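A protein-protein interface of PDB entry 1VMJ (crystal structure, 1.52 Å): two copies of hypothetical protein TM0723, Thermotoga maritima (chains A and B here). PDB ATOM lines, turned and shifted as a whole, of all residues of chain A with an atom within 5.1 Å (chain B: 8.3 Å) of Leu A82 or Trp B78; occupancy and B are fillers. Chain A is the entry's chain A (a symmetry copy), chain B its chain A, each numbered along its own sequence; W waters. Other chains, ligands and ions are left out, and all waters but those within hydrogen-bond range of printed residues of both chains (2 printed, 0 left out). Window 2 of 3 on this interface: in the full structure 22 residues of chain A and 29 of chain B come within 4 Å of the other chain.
The backbone carbonyl oxygen (O) of Leu A82 is in hydrogen-bond range of the indole nitrogen (NE1) of Trp B78 (2.8 Å).
Among the printed residues, pairs that only touch across the chains: Leu A105 with Phe B75, Thr A108 with Ile B109, Leu A105 with Trp B78, Thr A108 with Phe B75, Ile A109 with Trp B78, Thr A108 with Met B110 and Ala A83 with Trp B78.
Of the printed residues of chain B, Leu A82 touches Trp B78. Trp B78 touches just these residues of chain A: Leu A82 (2.8 Å), Ala A83 (3.9 Å), Leu A105 (3.5 Å) and Ile A109 (3.7 Å). Of the printed residues of chain B, Leu A105 touches Phe B75 and Trp B78. Of the printed residues of chain B, Ile A109 touches Trp B78 (3.7 Å). Leu B71 touches none of the printed residues of chain A. The nearest residue of chain B that does not touch Leu A82 is Leu B82 (4.2 Å).
Of the 18 printed residues of chain B, 4 touch a printed residue of chain A. Printed residues of chain A that touch a printed residue of chain B: Leu A82, Ala A83, Leu A105, Thr A108 and Ile A109. Along chain A the printed residues that touch a printed residue of chain B span positions 82 to 109. Among the printed residues, no Asp or Glu carboxylate lies within 4 Å of a Lys or Arg side-chain nitrogen of the other chain.
Leu A82 touches Trp B78, but with the chains exchanged Trp A78 does not touch Leu B82 (8.1 Å). Ala A83 touches Trp B78, but with the chains exchanged Trp A78 does not touch Ala B83 (12.2 Å). Ile A109 touches Trp B78, but with the chains exchanged Trp A78 does not touch Ile B109 (7.5 Å). Positions printed for both chains: 78, 79, 80, 81, 82, 83, 84 and 109. Of the 8 pairs that touch across the chains among the printed residues, none has its exchanged pair printed and touching as well.
Water W2 bridges the backbone carbonyl oxygen of Thr A108 (2.7 Å) and the backbone carbonyl oxygen of Met B110 (3.3 Å). Water W1 lies within hydrogen-bond range of the backbone carbonyl oxygen of Ile B109 and the backbone carbonyl oxygen of Ile A109.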
ATOM      1  N   TRP A  78     -18.416  13.665 -38.412  1.00  0.00           N
ATOM      2  CA  TRP A  78     -19.316  13.831 -37.260  1.00  0.00           C
ATOM      3  C   TRP A  78     -19.317  12.638 -36.331  1.00  0.00           C
ATOM      4  O   TRP A  78     -19.249  12.791 -35.124  1.00  0.00           O
ATOM      5  CB  TRP A  78     -20.701  14.063 -37.811  1.00  0.00           C
ATOM      6  CG  TRP A  78     -21.769  14.320 -36.854  1.00  0.00           C
ATOM      7  CD1 TRP A  78     -21.856  15.370 -35.996  1.00  0.00           C
ATOM      8  CD2 TRP A  78     -22.980  13.580 -36.708  1.00  0.00           C
ATOM      9  NE1 TRP A  78     -23.055  15.324 -35.308  1.00  0.00           N
ATOM     10  CE2 TRP A  78     -23.756  14.236 -35.737  1.00  0.00           C
ATOM     11  CE3 TRP A  78     -23.494  12.419 -37.311  1.00  0.00           C
ATOM     12  CZ2 TRP A  78     -25.010  13.772 -35.351  1.00  0.00           C
ATOM     13  CZ3 TRP A  78     -24.758  11.960 -36.917  1.00  0.00           C
ATOM     14  CH2 TRP A  78     -25.489  12.632 -35.949  1.00  0.00           C
ATOM     15  N   LEU A  79     -19.337  11.448 -36.897  1.00  0.00           N
ATOM     16  CA  LEU A  79     -19.325  10.251 -36.101  1.00  0.00           C
ATOM     17  C   LEU A  79     -18.005  10.077 -35.394  1.00  0.00           C
ATOM     18  O   LEU A  79     -17.963   9.532 -34.289  1.00  0.00           O
ATOM     19  CB  LEU A  79     -19.617   9.019 -36.964  1.00  0.00           C
ATOM     20  CG  LEU A  79     -21.042   8.910 -37.507  1.00  0.00           C
ATOM     21  CD1 LEU A  79     -21.166   7.877 -38.637  1.00  0.00           C
ATOM     22  CD2 LEU A  79     -21.998   8.574 -36.351  1.00  0.00           C
ATOM     23  N   GLU A  80     -16.915  10.507 -36.024  1.00  0.00           N
ATOM     24  CA  GLU A  80     -15.620  10.476 -35.361  1.00  0.00           C
ATOM     25  C   GLU A  80     -15.552  11.464 -34.199  1.00  0.00           C
ATOM     26  O   GLU A  80     -14.843  11.236 -33.207  1.00  0.00           O
ATOM     27  CB  GLU A  80     -14.472  10.717 -36.338  1.00  0.00           C
ATOM     28  CG  GLU A  80     -13.918   9.445 -36.950  1.00  0.00           C
ATOM     29  CD  GLU A  80     -13.077   8.663 -35.970  1.00  0.00           C
ATOM     30  OE1 GLU A  80     -11.867   8.955 -35.829  1.00  0.00           O
ATOM     31  OE2 GLU A  80     -13.622   7.745 -35.315  1.00  0.00           O
ATOM     32  N   LYS A  81     -16.250  12.581 -34.313  1.00  0.00           N
ATOM     33  CA  LYS A  81     -16.362  13.538 -33.228  1.00  0.00           C
ATOM     34  C   LYS A  81     -17.192  12.985 -32.086  1.00  0.00           C
ATOM     35  O   LYS A  81     -16.816  13.107 -30.935  1.00  0.00           O
ATOM     36  CB  LYS A  81     -16.931  14.853 -33.741  1.00  0.00           C
ATOM     37  CG  LYS A  81     -17.084  15.902 -32.653  1.00  0.00           C
ATOM     38  CD  LYS A  81     -17.334  17.300 -33.216  1.00  0.00           C
ATOM     39  N   LEU A  82     -18.322  12.376 -32.388  1.00  0.00           N
ATOM     40  CA  LEU A  82     -19.206  11.887 -31.340  1.00  0.00           C
ATOM     41  C   LEU A  82     -18.735  10.609 -30.685  1.00  0.00           C
ATOM     42  O   LEU A  82     -19.014  10.389 -29.498  1.00  0.00           O
ATOM     43  CB  LEU A  82     -20.592  11.644 -31.907  1.00  0.00           C
ATOM     44  CG  LEU A  82     -21.373  12.827 -32.448  1.00  0.00           C
ATOM     45  CD1 LEU A  82     -22.731  12.363 -32.888  1.00  0.00           C
ATOM     46  CD2 LEU A  82     -21.463  13.903 -31.412  1.00  0.00           C
ATOM     47  N   ALA A  83     -18.044   9.759 -31.455  1.00  0.00           N
ATOM     48  CA  ALA A  83     -17.635   8.432 -30.995  1.00  0.00           C
ATOM     49  C   ALA A  83     -16.301   8.040 -31.614  1.00  0.00           C
ATOM     50  O   ALA A  83     -16.237   7.187 -32.485  1.00  0.00           O
ATOM     51  CB  ALA A  83     -18.721   7.431 -31.358  1.00  0.00           C
ATOM     52  N   PRO A  84     -15.221   8.704 -31.189  1.00  0.00           N
ATOM     53  CA  PRO A  84     -13.911   8.506 -31.775  1.00  0.00           C
ATOM     54  C   PRO A  84     -13.406   7.079 -31.685  1.00  0.00           C
ATOM     55  O   PRO A  84     -13.536   6.434 -30.668  1.00  0.00           O
ATOM     56  CB  PRO A  84     -13.013   9.458 -30.988  1.00  0.00           C
ATOM     57  CG  PRO A  84     -13.766   9.786 -29.801  1.00  0.00           C
ATOM     58  CD  PRO A  84     -15.192   9.740 -30.159  1.00  0.00           C
ATOM     59  N   LEU A 105     -20.784   2.277 -30.818  1.00  0.00           N
ATOM     60  CA  LEU A 105     -21.298   3.635 -30.572  1.00  0.00           C
ATOM     61  C   LEU A 105     -21.759   4.344 -31.854  1.00  0.00           C
ATOM     62  O   LEU A 105     -22.853   4.895 -31.891  1.00  0.00           O
ATOM     63  CB  LEU A 105     -20.251   4.490 -29.805  1.00  0.00           C
ATOM     64  CG  LEU A 105     -19.713   3.861 -28.527  1.00  0.00           C
ATOM     65  CD1 LEU A 105     -18.757   4.825 -27.854  1.00  0.00           C
ATOM     66  CD2 LEU A 105     -20.771   3.391 -27.585  1.00  0.00           C
ATOM     67  N   THR A 108     -24.970   3.078 -33.083  1.00  0.00           N
ATOM     68  CA  THR A 108     -26.054   3.549 -32.251  1.00  0.00           C
ATOM     69  C   THR A 108     -26.568   4.899 -32.749  1.00  0.00           C
ATOM     70  O   THR A 108     -27.779   5.106 -32.828  1.00  0.00           O
ATOM     71  CB  THR A 108     -25.614   3.583 -30.791  1.00  0.00           C
ATOM     72  OG1 THR A 108     -25.233   2.267 -30.383  1.00  0.00           O
ATOM     73  CG2 THR A 108     -26.732   4.094 -29.896  1.00  0.00           C
ATOM     74  N   ILE A 109     -25.667   5.803 -33.106  1.00  0.00           N
ATOM     75  CA  ILE A 109     -26.087   7.079 -33.672  1.00  0.00           C
ATOM     76  C   ILE A 109     -26.878   6.905 -34.962  1.00  0.00           C
ATOM     77  O   ILE A 109     -27.941   7.503 -35.122  1.00  0.00           O
ATOM     78  CB  ILE A 109     -24.875   7.976 -33.931  1.00  0.00           C
ATOM     79  CG1 ILE A 109     -24.180   8.314 -32.607  1.00  0.00           C
ATOM     80  CG2 ILE A 109     -25.259   9.246 -34.676  1.00  0.00           C
ATOM     81  CD1 ILE A 109     -25.015   9.110 -31.645  1.00  0.00           C
ATOM     82  N   PHE B  30     -28.781  -1.194 -17.586  1.00  0.00           N
ATOM     83  CA  PHE B  30     -29.095  -1.962 -18.785  1.00  0.00           C
ATOM     84  C   PHE B  30     -29.510  -3.358 -18.350  1.00  0.00           C
ATOM     85  O   PHE B  30     -28.808  -3.992 -17.543  1.00  0.00           O
ATOM     86  CB  PHE B  30     -27.898  -2.040 -19.721  1.00  0.00           C
ATOM     87  CG  PHE B  30     -27.398  -0.696 -20.171  1.00  0.00           C
ATOM     88  CD1 PHE B  30     -28.153   0.099 -21.009  1.00  0.00           C
ATOM     89  CD2 PHE B  30     -26.150  -0.229 -19.764  1.00  0.00           C
ATOM     90  CE1 PHE B  30     -27.683   1.335 -21.426  1.00  0.00           C
ATOM     91  CE2 PHE B  30     -25.682   1.013 -20.175  1.00  0.00           C
ATOM     92  CZ  PHE B  30     -26.441   1.788 -21.004  1.00  0.00           C
ATOM     93  N   LEU B  71     -18.440  -2.876 -22.520  1.00  0.00           N
ATOM     94  CA  LEU B  71     -19.224  -2.034 -23.419  1.00  0.00           C
ATOM     95  C   LEU B  71     -20.342  -1.301 -22.701  1.00  0.00           C
ATOM     96  O   LEU B  71     -20.611  -0.143 -22.998  1.00  0.00           O
ATOM     97  CB  LEU B  71     -19.753  -2.843 -24.595  1.00  0.00           C
ATOM     98  CG  LEU B  71     -20.392  -2.007 -25.695  1.00  0.00           C
ATOM     99  CD1 LEU B  71     -19.294  -1.188 -26.371  1.00  0.00           C
ATOM    100  CD2 LEU B  71     -21.119  -2.830 -26.746  1.00  0.00           C
ATOM    101  N   HIS B  72     -20.981  -1.963 -21.733  1.00  0.00           N
ATOM    102  CA  HIS B  72     -22.000  -1.296 -20.927  1.00  0.00           C
ATOM    103  C   HIS B  72     -21.430  -0.107 -20.187  1.00  0.00           C
ATOM    104  O   HIS B  72     -22.038   0.961 -20.169  1.00  0.00           O
ATOM    105  CB  HIS B  72     -22.642  -2.270 -19.968  1.00  0.00           C
ATOM    106  CG  HIS B  72     -23.443  -3.318 -20.661  1.00  0.00           C
ATOM    107  ND1 HIS B  72     -23.999  -4.384 -19.994  1.00  0.00           N
ATOM    108  CD2 HIS B  72     -23.769  -3.480 -21.968  1.00  0.00           C
ATOM    109  CE1 HIS B  72     -24.648  -5.151 -20.852  1.00  0.00           C
ATOM    110  NE2 HIS B  72     -24.526  -4.626 -22.057  1.00  0.00           N
ATOM    111  N   HIS B  73     -20.245  -0.293 -19.617  1.00  0.00           N
ATOM    112  CA  HIS B  73     -19.532   0.809 -19.013  1.00  0.00           C
ATOM    113  C   HIS B  73     -19.258   1.922 -20.033  1.00  0.00           C
ATOM    114  O   HIS B  73     -19.497   3.100 -19.767  1.00  0.00           O
ATOM    115  CB  HIS B  73     -18.225   0.334 -18.374  1.00  0.00           C
ATOM    116  CG  HIS B  73     -17.377   1.453 -17.876  1.00  0.00           C
ATOM    117  ND1 HIS B  73     -17.548   2.016 -16.630  1.00  0.00           N
ATOM    118  CD2 HIS B  73     -16.379   2.147 -18.472  1.00  0.00           C
ATOM    119  CE1 HIS B  73     -16.671   2.994 -16.472  1.00  0.00           C
ATOM    120  NE2 HIS B  73     -15.941   3.085 -17.571  1.00  0.00           N
ATOM    121  N   ASP B  74     -18.806   1.546 -21.223  1.00  0.00           N
ATOM    122  CA  ASP B  74     -18.535   2.535 -22.259  1.00  0.00           C
ATOM    123  C   ASP B  74     -19.787   3.318 -22.662  1.00  0.00           C
ATOM    124  O   ASP B  74     -19.720   4.527 -22.829  1.00  0.00           O
ATOM    125  CB  ASP B  74     -17.936   1.861 -23.499  1.00  0.00           C
ATOM    126  CG  ASP B  74     -16.586   1.193 -23.222  1.00  0.00           C
ATOM    127  OD1 ASP B  74     -15.872   1.639 -22.289  1.00  0.00           O
ATOM    128  OD2 ASP B  74     -16.236   0.234 -23.928  1.00  0.00           O
ATOM    129  N   PHE B  75     -20.935   2.657 -22.775  1.00  0.00           N
ATOM    130  CA  PHE B  75     -22.182   3.370 -23.085  1.00  0.00           C
ATOM    131  C   PHE B  75     -22.517   4.376 -21.971  1.00  0.00           C
ATOM    132  O   PHE B  75     -22.946   5.487 -22.242  1.00  0.00           O
ATOM    133  CB  PHE B  75     -23.372   2.404 -23.301  1.00  0.00           C
ATOM    134  CG  PHE B  75     -23.484   1.874 -24.696  1.00  0.00           C
ATOM    135  CD1 PHE B  75     -23.775   2.709 -25.751  1.00  0.00           C
ATOM    136  CD2 PHE B  75     -23.371   0.522 -24.936  1.00  0.00           C
ATOM    137  CE1 PHE B  75     -23.923   2.188 -27.037  1.00  0.00           C
ATOM    138  CE2 PHE B  75     -23.505   0.015 -26.213  1.00  0.00           C
ATOM    139  CZ  PHE B  75     -23.780   0.841 -27.252  1.00  0.00           C
ATOM    140  N   GLU B  76     -22.359   3.968 -20.721  1.00  0.00           N
ATOM    141  CA  GLU B  76     -22.622   4.870 -19.591  1.00  0.00           C
ATOM    142  C   GLU B  76     -21.779   6.132 -19.691  1.00  0.00           C
ATOM    143  O   GLU B  76     -22.286   7.269 -19.581  1.00  0.00           O
ATOM    144  CB  GLU B  76     -22.387   4.135 -18.264  1.00  0.00           C
ATOM    145  CG  GLU B  76     -22.156   5.030 -17.054  1.00  0.00           C
ATOM    146  CD  GLU B  76     -23.369   5.816 -16.587  1.00  0.00           C
ATOM    147  OE1 GLU B  76     -24.511   5.480 -16.940  1.00  0.00           O
ATOM    148  OE2 GLU B  76     -23.164   6.785 -15.818  1.00  0.00           O
ATOM    149  N   VAL B  77     -20.488   5.941 -19.895  1.00  0.00           N
ATOM    150  CA  VAL B  77     -19.556   7.069 -20.005  1.00  0.00           C
ATOM    151  C   VAL B  77     -19.913   7.963 -21.210  1.00  0.00           C
ATOM    152  O   VAL B  77     -19.926   9.180 -21.123  1.00  0.00           O
ATOM    153  CB  VAL B  77     -18.095   6.567 -20.127  1.00  0.00           C
ATOM    154  CG1 VAL B  77     -17.161   7.704 -20.494  1.00  0.00           C
ATOM    155  CG2 VAL B  77     -17.674   5.880 -18.827  1.00  0.00           C
ATOM    156  N   TRP B  78     -20.217   7.331 -22.336  1.00  0.00           N
ATOM    157  CA  TRP B  78     -20.525   8.055 -23.578  1.00  0.00           C
ATOM    158  C   TRP B  78     -21.813   8.843 -23.501  1.00  0.00           C
ATOM    159  O   TRP B  78     -21.866   9.989 -23.910  1.00  0.00           O
ATOM    160  CB  TRP B  78     -20.607   7.029 -24.681  1.00  0.00           C
ATOM    161  CG  TRP B  78     -20.844   7.515 -26.034  1.00  0.00           C
ATOM    162  CD1 TRP B  78     -20.034   8.332 -26.757  1.00  0.00           C
ATOM    163  CD2 TRP B  78     -21.913   7.141 -26.900  1.00  0.00           C
ATOM    164  NE1 TRP B  78     -20.544   8.503 -28.030  1.00  0.00           N
ATOM    165  CE2 TRP B  78     -21.693   7.775 -28.134  1.00  0.00           C
ATOM    166  CE3 TRP B  78     -23.046   6.322 -26.755  1.00  0.00           C
ATOM    167  CZ2 TRP B  78     -22.560   7.623 -29.212  1.00  0.00           C
ATOM    168  CZ3 TRP B  78     -23.912   6.173 -27.846  1.00  0.00           C
ATOM    169  CH2 TRP B  78     -23.663   6.822 -29.046  1.00  0.00           C
ATOM    170  N   LEU B  79     -22.838   8.246 -22.926  1.00  0.00           N
ATOM    171  CA  LEU B  79     -24.104   8.915 -22.792  1.00  0.00           C
ATOM    172  C   LEU B  79     -24.013  10.063 -21.820  1.00  0.00           C
ATOM    173  O   LEU B  79     -24.711  11.066 -21.982  1.00  0.00           O
ATOM    174  CB  LEU B  79     -25.192   7.936 -22.338  1.00  0.00           C
ATOM    175  CG  LEU B  79     -25.607   6.882 -23.365  1.00  0.00           C
ATOM    176  CD1 LEU B  79     -26.413   5.734 -22.739  1.00  0.00           C
ATOM    177  CD2 LEU B  79     -26.405   7.560 -24.490  1.00  0.00           C
ATOM    178  N   GLU B  80     -23.183   9.926 -20.789  1.00  0.00           N
ATOM    179  CA  GLU B  80     -22.957  11.033 -19.872  1.00  0.00           C
ATOM    180  C   GLU B  80     -22.216  12.187 -20.543  1.00  0.00           C
ATOM    181  O   GLU B  80     -22.404  13.360 -20.187  1.00  0.00           O
ATOM    182  CB  GLU B  80     -22.227  10.588 -18.608  1.00  0.00           C
ATOM    183  CG  GLU B  80     -23.154  10.164 -17.486  1.00  0.00           C
ATOM    184  CD  GLU B  80     -23.823  11.345 -16.826  1.00  0.00           C
ATOM    185  OE1 GLU B  80     -23.226  11.956 -15.910  1.00  0.00           O
ATOM    186  OE2 GLU B  80     -24.961  11.687 -17.223  1.00  0.00           O
ATOM    187  N   LYS B  81     -21.345  11.877 -21.489  1.00  0.00           N
ATOM    188  CA  LYS B  81     -20.671  12.890 -22.280  1.00  0.00           C
ATOM    189  C   LYS B  81     -21.634  13.591 -23.218  1.00  0.00           C
ATOM    190  O   LYS B  81     -21.617  14.803 -23.326  1.00  0.00           O
ATOM    191  CB  LYS B  81     -19.505  12.273 -23.041  1.00  0.00           C
ATOM    192  CG  LYS B  81     -18.757  13.278 -23.902  1.00  0.00           C
ATOM    193  CD  LYS B  81     -17.413  12.743 -24.392  1.00  0.00           C
ATOM    194  N   LEU B  82     -22.479  12.843 -23.902  1.00  0.00           N
ATOM    195  CA  LEU B  82     -23.379  13.442 -24.876  1.00  0.00           C
ATOM    196  C   LEU B  82     -24.564  14.152 -24.262  1.00  0.00           C
ATOM    197  O   LEU B  82     -25.063  15.126 -24.843  1.00  0.00           O
ATOM    198  CB  LEU B  82     -23.906  12.372 -25.815  1.00  0.00           C
ATOM    199  CG  LEU B  82     -22.921  11.641 -26.708  1.00  0.00           C
ATOM    200  CD1 LEU B  82     -23.669  10.687 -27.593  1.00  0.00           C
ATOM    201  CD2 LEU B  82     -22.120  12.623 -27.504  1.00  0.00           C
ATOM    202  N   ALA B  83     -25.027  13.659 -23.107  1.00  0.00           N
ATOM    203  CA  ALA B  83     -26.241  14.164 -22.464  1.00  0.00           C
ATOM    204  C   ALA B  83     -26.115  14.084 -20.949  1.00  0.00           C
ATOM    205  O   ALA B  83     -26.743  13.257 -20.308  1.00  0.00           O
ATOM    206  CB  ALA B  83     -27.429  13.355 -22.957  1.00  0.00           C
ATOM    207  N   PRO B  84     -25.256  14.929 -20.370  1.00  0.00           N
ATOM    208  CA  PRO B  84     -24.960  14.881 -18.952  1.00  0.00           C
ATOM    209  C   PRO B  84     -26.174  15.076 -18.064  1.00  0.00           C
ATOM    210  O   PRO B  84     -27.000  15.926 -18.314  1.00  0.00           O
ATOM    211  CB  PRO B  84     -23.947  16.006 -18.754  1.00  0.00           C
ATOM    212  CG  PRO B  84     -24.067  16.829 -19.933  1.00  0.00           C
ATOM    213  CD  PRO B  84     -24.456  15.949 -21.046  1.00  0.00           C
ATOM    214  N   LYS B 106     -30.729  10.911 -23.328  1.00  0.00           N
ATOM    215  CA  LYS B 106     -30.031   9.634 -23.389  1.00  0.00           C
ATOM    216  C   LYS B 106     -30.859   8.597 -24.149  1.00  0.00           C
ATOM    217  O   LYS B 106     -30.345   7.854 -24.981  1.00  0.00           O
ATOM    218  CB  LYS B 106     -29.681   9.132 -21.980  1.00  0.00           C
ATOM    219  CG  LYS B 106     -28.583   9.868 -21.261  1.00  0.00           C
ATOM    220  CD  LYS B 106     -28.278   9.173 -19.940  1.00  0.00           C
ATOM    221  CE  LYS B 106     -27.001   9.682 -19.281  1.00  0.00           C
ATOM    222  NZ  LYS B 106     -27.152  11.067 -18.825  1.00  0.00           N
ATOM    223  N   ILE B 109     -30.648   8.981 -27.904  1.00  0.00           N
ATOM    224  CA  ILE B 109     -29.466   8.372 -28.503  1.00  0.00           C
ATOM    225  C   ILE B 109     -29.628   6.869 -28.694  1.00  0.00           C
ATOM    226  O   ILE B 109     -29.342   6.347 -29.771  1.00  0.00           O
ATOM    227  CB  ILE B 109     -28.228   8.650 -27.650  1.00  0.00           C
ATOM    228  CG1 ILE B 109     -27.946  10.157 -27.609  1.00  0.00           C
ATOM    229  CG2 ILE B 109     -27.011   7.890 -28.153  1.00  0.00           C
ATOM    230  CD1 ILE B 109     -27.610  10.768 -28.940  1.00  0.00           C
ATOM    231  N   MET B 110     -30.065   6.165 -27.662  1.00  0.00           N
ATOM    232  CA  MET B 110     -30.100   4.701 -27.726  1.00  0.00           C
ATOM    233  C   MET B 110     -31.282   4.199 -28.554  1.00  0.00           C
ATOM    234  O   MET B 110     -31.236   3.089 -29.121  1.00  0.00           O
ATOM    235  CB  MET B 110     -30.138   4.093 -26.330  1.00  0.00           C
ATOM    236  CG  MET B 110     -28.949   4.360 -25.452  1.00  0.00           C
ATOM    237  SD  MET B 110     -27.373   3.949 -26.158  1.00  0.00           S
ATOM    238  CE  MET B 110     -27.583   2.220 -26.393  1.00  0.00           C
HETATM  239  O   HOH W   1     -29.421   8.402 -32.331  1.00  0.00           O
HETATM  240  O   HOH W   2     -29.734   3.349 -32.045  1.00  0.00           O
